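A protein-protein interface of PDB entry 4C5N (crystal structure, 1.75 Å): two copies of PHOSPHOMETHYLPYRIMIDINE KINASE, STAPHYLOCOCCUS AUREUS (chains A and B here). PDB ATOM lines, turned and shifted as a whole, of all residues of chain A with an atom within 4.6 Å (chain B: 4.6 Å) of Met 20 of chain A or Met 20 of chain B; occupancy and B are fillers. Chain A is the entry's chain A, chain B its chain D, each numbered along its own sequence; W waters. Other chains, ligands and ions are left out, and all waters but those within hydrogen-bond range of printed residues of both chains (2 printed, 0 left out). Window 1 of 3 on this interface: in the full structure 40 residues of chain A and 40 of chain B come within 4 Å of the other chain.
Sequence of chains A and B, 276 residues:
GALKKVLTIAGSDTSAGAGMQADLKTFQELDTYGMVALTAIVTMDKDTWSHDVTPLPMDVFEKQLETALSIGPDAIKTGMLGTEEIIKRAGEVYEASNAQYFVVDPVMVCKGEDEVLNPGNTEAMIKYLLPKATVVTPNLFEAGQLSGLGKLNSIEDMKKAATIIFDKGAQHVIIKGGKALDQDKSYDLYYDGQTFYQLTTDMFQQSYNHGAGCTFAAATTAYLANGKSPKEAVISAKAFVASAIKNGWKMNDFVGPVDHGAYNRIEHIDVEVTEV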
ATOM      1  N   THR A   8     -16.725 -26.747 -16.739  1.00  0.00           N
ATOM      2  CA  THR A   8     -17.725 -27.707 -17.156  1.00  0.00           C
ATOM      3  C   THR A   8     -17.562 -27.979 -18.671  1.00  0.00           C
ATOM      4  O   THR A   8     -17.367 -27.033 -19.460  1.00  0.00           O
ATOM      5  CB  THR A   8     -19.169 -27.259 -16.870  1.00  0.00           C
ATOM      6  OG1 THR A   8     -20.040 -28.346 -17.206  1.00  0.00           O
ATOM      7  CG2 THR A   8     -19.568 -26.031 -17.666  1.00  0.00           C
ATOM      8  N   ALA A  10     -19.634 -29.368 -21.475  1.00  0.00           N
ATOM      9  CA  ALA A  10     -21.087 -29.409 -21.468  1.00  0.00           C
ATOM     10  C   ALA A  10     -21.699 -28.756 -22.708  1.00  0.00           C
ATOM     11  O   ALA A  10     -21.014 -27.973 -23.405  1.00  0.00           O
ATOM     12  CB  ALA A  10     -21.513 -28.687 -20.210  1.00  0.00           C
ATOM     13  N   GLY A  11     -22.974 -29.030 -22.995  1.00  0.00           N
ATOM     14  CA  GLY A  11     -23.679 -28.308 -24.064  1.00  0.00           C
ATOM     15  C   GLY A  11     -24.407 -27.084 -23.559  1.00  0.00           C
ATOM     16  O   GLY A  11     -24.602 -26.897 -22.340  1.00  0.00           O
ATOM     17  N   SER A  12     -24.850 -26.265 -24.498  1.00  0.00           N
ATOM     18  CA  SER A  12     -25.665 -25.178 -24.229  1.00  0.00           C
ATOM     19  C   SER A  12     -27.152 -25.544 -24.309  1.00  0.00           C
ATOM     20  O   SER A  12     -27.607 -26.017 -25.344  1.00  0.00           O
ATOM     21  CB  SER A  12     -25.330 -24.024 -25.177  1.00  0.00           C
ATOM     22  OG  SER A  12     -26.267 -22.994 -24.979  1.00  0.00           O
ATOM     23  N   ALA A  18     -30.826 -25.541 -17.767  1.00  0.00           N
ATOM     24  CA  ALA A  18     -29.900 -26.679 -17.631  1.00  0.00           C
ATOM     25  C   ALA A  18     -28.681 -26.422 -18.388  1.00  0.00           C
ATOM     26  O   ALA A  18     -28.389 -25.265 -18.773  1.00  0.00           O
ATOM     27  CB  ALA A  18     -30.567 -27.968 -18.112  1.00  0.00           C
ATOM     28  N   GLY A  19     -27.867 -27.478 -18.503  1.00  0.00           N
ATOM     29  CA  GLY A  19     -26.701 -27.372 -19.316  1.00  0.00           C
ATOM     30  C   GLY A  19     -25.607 -26.501 -18.691  1.00  0.00           C
ATOM     31  O   GLY A  19     -25.570 -26.270 -17.450  1.00  0.00           O
ATOM     32  N   MET A  20     -24.799 -25.905 -19.588  1.00  0.00           N
ATOM     33  CA  MET A  20     -23.657 -25.091 -19.218  1.00  0.00           C
ATOM     34  C   MET A  20     -24.237 -23.827 -18.543  1.00  0.00           C
ATOM     35  O   MET A  20     -23.594 -23.252 -17.653  1.00  0.00           O
ATOM     36  CB  MET A  20     -22.744 -24.785 -20.409  1.00  0.00           C
ATOM     37  CG  MET A  20     -23.388 -23.870 -21.460  1.00  0.00           C
ATOM     38  SD  MET A  20     -23.039 -22.128 -21.089  1.00  0.00           S
ATOM     39  CE  MET A  20     -23.702 -21.394 -22.589  1.00  0.00           C
ATOM     40  N   GLN A  21     -25.455 -23.425 -18.932  1.00  0.00           N
ATOM     41  CA  GLN A  21     -26.103 -22.318 -18.250  1.00  0.00           C
ATOM     42  C   GLN A  21     -26.388 -22.555 -16.792  1.00  0.00           C
ATOM     43  O   GLN A  21     -25.976 -21.738 -15.933  1.00  0.00           O
ATOM     44  CB  GLN A  21     -27.384 -21.971 -18.943  1.00  0.00           C
ATOM     45  CG  GLN A  21     -27.196 -21.301 -20.272  1.00  0.00           C
ATOM     46  CD  GLN A  21     -27.072 -22.199 -21.439  1.00  0.00           C
ATOM     47  OE1 GLN A  21     -26.718 -23.375 -21.335  1.00  0.00           O
ATOM     48  NE2 GLN A  21     -27.306 -21.621 -22.606  1.00  0.00           N
ATOM     49  N   ALA A  22     -27.005 -23.671 -16.455  1.00  0.00           N
ATOM     50  CA  ALA A  22     -27.128 -24.105 -15.049  1.00  0.00           C
ATOM     51  C   ALA A  22     -25.766 -24.187 -14.385  1.00  0.00           C
ATOM     52  O   ALA A  22     -25.609 -23.778 -13.185  1.00  0.00           O
ATOM     53  CB  ALA A  22     -27.773 -25.466 -14.921  1.00  0.00           C
ATOM     54  N   ASP A  23     -24.811 -24.728 -15.089  1.00  0.00           N
ATOM     55  CA  ASP A  23     -23.503 -24.892 -14.475  1.00  0.00           C
ATOM     56  C   ASP A  23     -22.830 -23.519 -14.093  1.00  0.00           C
ATOM     57  O   ASP A  23     -22.339 -23.296 -12.967  1.00  0.00           O
ATOM     58  CB  ASP A  23     -22.540 -25.678 -15.346  1.00  0.00           C
ATOM     59  CG  ASP A  23     -22.992 -27.087 -15.685  1.00  0.00           C
ATOM     60  OD1 ASP A  23     -23.869 -27.658 -14.924  1.00  0.00           O
ATOM     61  OD2 ASP A  23     -22.515 -27.658 -16.767  1.00  0.00           O
ATOM     62  N   LEU A  24     -22.692 -22.644 -15.059  1.00  0.00           N
ATOM     63  CA  LEU A  24     -22.085 -21.300 -14.825  1.00  0.00           C
ATOM     64  C   LEU A  24     -22.886 -20.502 -13.797  1.00  0.00           C
ATOM     65  O   LEU A  24     -22.320 -19.870 -12.945  1.00  0.00           O
ATOM     66  CB  LEU A  24     -22.152 -20.540 -16.132  1.00  0.00           C
ATOM     67  CG  LEU A  24     -21.274 -21.023 -17.254  1.00  0.00           C
ATOM     68  CD1 LEU A  24     -21.305 -19.958 -18.326  1.00  0.00           C
ATOM     69  CD2 LEU A  24     -19.849 -21.320 -16.710  1.00  0.00           C
ATOM     70  N   VAL A  36     -16.447 -22.886 -19.252  1.00  0.00           N
ATOM     71  CA  VAL A  36     -17.064 -23.909 -20.023  1.00  0.00           C
ATOM     72  C   VAL A  36     -16.319 -24.196 -21.318  1.00  0.00           C
ATOM     73  O   VAL A  36     -15.915 -23.310 -22.026  1.00  0.00           O
ATOM     74  CB  VAL A  36     -18.526 -23.525 -20.380  1.00  0.00           C
ATOM     75  CG1 VAL A  36     -18.593 -22.175 -21.071  1.00  0.00           C
ATOM     76  CG2 VAL A  36     -19.247 -24.608 -21.184  1.00  0.00           C
ATOM     77  N   LEU A  38     -17.650 -25.849 -24.679  1.00  0.00           N
ATOM     78  CA  LEU A  38     -18.989 -26.212 -25.234  1.00  0.00           C
ATOM     79  C   LEU A  38     -18.886 -27.332 -26.236  1.00  0.00           C
ATOM     80  O   LEU A  38     -18.068 -27.297 -27.170  1.00  0.00           O
ATOM     81  CB  LEU A  38     -19.648 -25.050 -25.948  1.00  0.00           C
ATOM     82  CG  LEU A  38     -19.954 -23.795 -25.155  1.00  0.00           C
ATOM     83  CD1 LEU A  38     -19.929 -22.520 -26.015  1.00  0.00           C
ATOM     84  CD2 LEU A  38     -21.217 -23.897 -24.376  1.00  0.00           C
ATOM     85  N   THR B   8     -28.613 -12.182 -23.615  1.00  0.00           N
ATOM     86  CA  THR B   8     -27.479 -11.611 -24.280  1.00  0.00           C
ATOM     87  C   THR B   8     -27.280 -12.321 -25.622  1.00  0.00           C
ATOM     88  O   THR B   8     -27.436 -13.527 -25.730  1.00  0.00           O
ATOM     89  CB  THR B   8     -26.211 -11.745 -23.465  1.00  0.00           C
ATOM     90  OG1 THR B   8     -25.172 -11.006 -24.127  1.00  0.00           O
ATOM     91  CG2 THR B   8     -25.773 -13.159 -23.262  1.00  0.00           C
ATOM     92  N   ALA B  10     -24.378 -12.829 -28.020  1.00  0.00           N
ATOM     93  CA  ALA B  10     -22.989 -12.704 -27.714  1.00  0.00           C
ATOM     94  C   ALA B  10     -22.170 -13.914 -28.036  1.00  0.00           C
ATOM     95  O   ALA B  10     -22.721 -15.014 -28.274  1.00  0.00           O
ATOM     96  CB  ALA B  10     -22.880 -12.377 -26.207  1.00  0.00           C
ATOM     97  N   GLY B  11     -20.868 -13.738 -28.054  1.00  0.00           N
ATOM     98  CA  GLY B  11     -19.939 -14.819 -28.299  1.00  0.00           C
ATOM     99  C   GLY B  11     -19.490 -15.426 -26.980  1.00  0.00           C
ATOM    100  O   GLY B  11     -19.683 -14.826 -25.917  1.00  0.00           O
ATOM    101  N   SER B  12     -18.854 -16.580 -27.058  1.00  0.00           N
ATOM    102  CA  SER B  12     -18.288 -17.212 -25.924  1.00  0.00           C
ATOM    103  C   SER B  12     -16.833 -16.841 -25.764  1.00  0.00           C
ATOM    104  O   SER B  12     -16.064 -17.001 -26.659  1.00  0.00           O
ATOM    105  CB  SER B  12     -18.434 -18.724 -26.094  1.00  0.00           C
ATOM    106  OG  SER B  12     -17.775 -19.410 -25.037  1.00  0.00           O
ATOM    107  N   ALA B  18     -15.011 -12.389 -19.974  1.00  0.00           N
ATOM    108  CA  ALA B  18     -15.817 -11.522 -20.787  1.00  0.00           C
ATOM    109  C   ALA B  18     -16.884 -12.298 -21.561  1.00  0.00           C
ATOM    110  O   ALA B  18     -17.251 -13.430 -21.215  1.00  0.00           O
ATOM    111  CB  ALA B  18     -14.966 -10.695 -21.720  1.00  0.00           C
ATOM    112  N   GLY B  19     -17.399 -11.693 -22.617  1.00  0.00           N
ATOM    113  CA  GLY B  19     -18.349 -12.395 -23.466  1.00  0.00           C
ATOM    114  C   GLY B  19     -19.591 -12.825 -22.719  1.00  0.00           C
ATOM    115  O   GLY B  19     -19.948 -12.228 -21.688  1.00  0.00           O
ATOM    116  N   MET B  20     -20.221 -13.885 -23.207  1.00  0.00           N
ATOM    117  CA  MET B  20     -21.455 -14.388 -22.635  1.00  0.00           C
ATOM    118  C   MET B  20     -21.270 -14.922 -21.250  1.00  0.00           C
ATOM    119  O   MET B  20     -22.215 -14.928 -20.473  1.00  0.00           O
ATOM    120  CB  MET B  20     -22.116 -15.400 -23.509  1.00  0.00           C
ATOM    121  CG  MET B  20     -21.398 -16.693 -23.668  1.00  0.00           C
ATOM    122  SD  MET B  20     -21.913 -17.921 -22.449  1.00  0.00           S
ATOM    123  CE  MET B  20     -20.903 -19.260 -22.968  1.00  0.00           C
ATOM    124  N   GLN B  21     -20.069 -15.386 -20.966  1.00  0.00           N
ATOM    125  CA  GLN B  21     -19.704 -15.750 -19.632  1.00  0.00           C
ATOM    126  C   GLN B  21     -19.852 -14.605 -18.607  1.00  0.00           C
ATOM    127  O   GLN B  21     -20.543 -14.757 -17.603  1.00  0.00           O
ATOM    128  CB  GLN B  21     -18.303 -16.264 -19.588  1.00  0.00           C
ATOM    129  CG  GLN B  21     -18.168 -17.642 -20.149  1.00  0.00           C
ATOM    130  CD  GLN B  21     -17.892 -17.694 -21.592  1.00  0.00           C
ATOM    131  OE1 GLN B  21     -18.201 -16.777 -22.355  1.00  0.00           O
ATOM    132  NE2 GLN B  21     -17.485 -18.821 -22.010  1.00  0.00           N
ATOM    133  N   ALA B  22     -19.183 -13.465 -18.839  1.00  0.00           N
ATOM    134  CA  ALA B  22     -19.424 -12.267 -17.988  1.00  0.00           C
ATOM    135  C   ALA B  22     -20.904 -11.881 -17.933  1.00  0.00           C
ATOM    136  O   ALA B  22     -21.390 -11.461 -16.888  1.00  0.00           O
ATOM    137  CB  ALA B  22     -18.579 -11.083 -18.507  1.00  0.00           C
ATOM    138  N   ASP B  23     -21.621 -12.087 -19.027  1.00  0.00           N
ATOM    139  CA  ASP B  23     -23.023 -11.650 -19.055  1.00  0.00           C
ATOM    140  C   ASP B  23     -23.951 -12.500 -18.144  1.00  0.00           C
ATOM    141  O   ASP B  23     -24.670 -11.988 -17.238  1.00  0.00           O
ATOM    142  CB  ASP B  23     -23.538 -11.730 -20.513  1.00  0.00           C
ATOM    143  CG  ASP B  23     -22.898 -10.698 -21.474  1.00  0.00           C
ATOM    144  OD1 ASP B  23     -22.270  -9.726 -20.987  1.00  0.00           O
ATOM    145  OD2 ASP B  23     -22.988 -10.914 -22.731  1.00  0.00           O
ATOM    146  N   LEU B  24     -23.835 -13.831 -18.297  1.00  0.00           N
ATOM    147  CA  LEU B  24     -24.621 -14.749 -17.501  1.00  0.00           C
ATOM    148  C   LEU B  24     -24.240 -14.627 -16.046  1.00  0.00           C
ATOM    149  O   LEU B  24     -25.095 -14.735 -15.204  1.00  0.00           O
ATOM    150  CB  LEU B  24     -24.479 -16.183 -17.946  1.00  0.00           C
ATOM    151  CG  LEU B  24     -24.933 -16.584 -19.349  1.00  0.00           C
ATOM    152  CD1 LEU B  24     -24.533 -18.052 -19.513  1.00  0.00           C
ATOM    153  CD2 LEU B  24     -26.369 -16.324 -19.513  1.00  0.00           C
ATOM    154  N   VAL B  36     -28.676 -16.766 -23.275  1.00  0.00           N
ATOM    155  CA  VAL B  36     -27.757 -16.416 -24.337  1.00  0.00           C
ATOM    156  C   VAL B  36     -28.168 -17.027 -25.654  1.00  0.00           C
ATOM    157  O   VAL B  36     -28.580 -18.182 -25.736  1.00  0.00           O
ATOM    158  CB  VAL B  36     -26.283 -16.779 -24.016  1.00  0.00           C
ATOM    159  CG1 VAL B  36     -26.166 -18.222 -23.619  1.00  0.00           C
ATOM    160  CG2 VAL B  36     -25.349 -16.404 -25.161  1.00  0.00           C
ATOM    161  N   LEU B  38     -25.749 -17.654 -28.795  1.00  0.00           N
ATOM    162  CA  LEU B  38     -24.329 -17.656 -29.117  1.00  0.00           C
ATOM    163  C   LEU B  38     -24.035 -17.302 -30.577  1.00  0.00           C
ATOM    164  O   LEU B  38     -24.623 -17.853 -31.509  1.00  0.00           O
ATOM    165  CB  LEU B  38     -23.735 -19.050 -28.819  1.00  0.00           C
ATOM    166  CG  LEU B  38     -23.839 -19.447 -27.350  1.00  0.00           C
ATOM    167  CD1 LEU B  38     -23.766 -20.944 -27.176  1.00  0.00           C
ATOM    168  CD2 LEU B  38     -22.762 -18.703 -26.539  1.00  0.00           C
HETATM  169  O   HOH W   1     -29.210 -19.503 -23.505  1.00  0.00           O
HETATM  170  O   HOH W   2     -15.479 -20.634 -20.945  1.00  0.00           O
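Met 20 of chain A touches one residue of chain B.
Of the printed residues of chain B, Leu 24 of chain A touches Leu 24.
Of the printed residues of chain A, Ser 12 of chain B touches Leu 38 (3.9 Å).
Met 20 of chain B touches just one residue of chain A: Met 20 (3.5 Å).
Printed residues of chain A within 4 Å of Val 36 of chain B: Gln 21.
The nearest residue of chain B that does not touch Met 20 of chain A is Val 36 of chain B (4.1 Å).
The nearest residue of chain A that does not touch Met 20 of chain B is Val 36 of chain A (4.2 Å).
The nearest printed residue of chain B that does not touch Ser 12 of chain A is Val 36 of chain B (5.0 Å).
OG of Ser 12 of chain A touches CD1 of Leu 38 of chain B, at 3.9 Å.
CE of Met 20 of chain A touches CE of Met 20 of chain B (3.5 Å).
NE2 of Gln 21 of chain A touches CG1 of Val 36 of chain B (3.7 Å).
Leu 24 of chain A touches Leu 24 of chain B (CD1 to CD1, 3.9 Å).
Val 36 of chain A touches Gln 21 of chain B (CG1 to NE2, 3.7 Å).
Ser 12 of chain B touches Leu 38 of chain A.
Ser 12 of chain A touches Leu 38 of chain B, and with the chains exchanged Leu 38 of chain A touches Ser 12 of chain B.
Met 20 of chain B touches its own counterpart, Met 20 of chain A.
Gln 21 of chain A touches Val 36 of chain B, and with the chains exchanged Val 36 of chain A touches Gln 21 of chain B.
Leu 24 of chain A touches its own counterpart, Leu 24 of chain B.
Positions printed for both chains: 8, 10, 11, 12, 18, 19, 20, 21, 22, 23, 24, 36 and 38.
Hydrophobic or aromatic side chains of chain A that line the printed part of chain B: Met 20, Leu 24, Val 36 and Leu 38.
Along chain A the printed residues that touch a printed residue of chain B span positions 12 to 38.
Hydrophobic or aromatic side chains of chain B that line the printed part of chain A: Met 20, Leu 24, Val 36 and Leu 38.
Among the printed residues, no Asp or Glu carboxylate lies within 4 Å of a Lys or Arg side-chain nitrogen of the other chain.
Water W1 bridges O of Val 36 of chain B (2.7 Å) and NE2 of Gln 21 of chain A (3.0 Å).
Water W2 lies within hydrogen-bond range of the side-chain amide nitrogen of Gln 21 of chain B (2.9 Å) and the backbone carbonyl oxygen of Val 36 of chain A (2.9 Å).
The side-chain hydroxyl (OG) of Ser 12 of chain B is in hydrogen-bond range of the side-chain amide nitrogen (NE2) of Gln 21 of chain B.
O of Gly 11 of chain B lies within hydrogen-bond range of N of Met 20 of chain B (2.9 Å).
The backbone NH (N) of Met 20 of chain A sits at hydrogen-bond distance from the backbone carbonyl oxygen (O) of Gly 11 of chain A (2.9 Å).
The side-chain amide nitrogen (NE2) of Gln 21 of chain A lies within hydrogen-bond range of the side-chain hydroxyl (OG) of Ser 12 of chain A.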
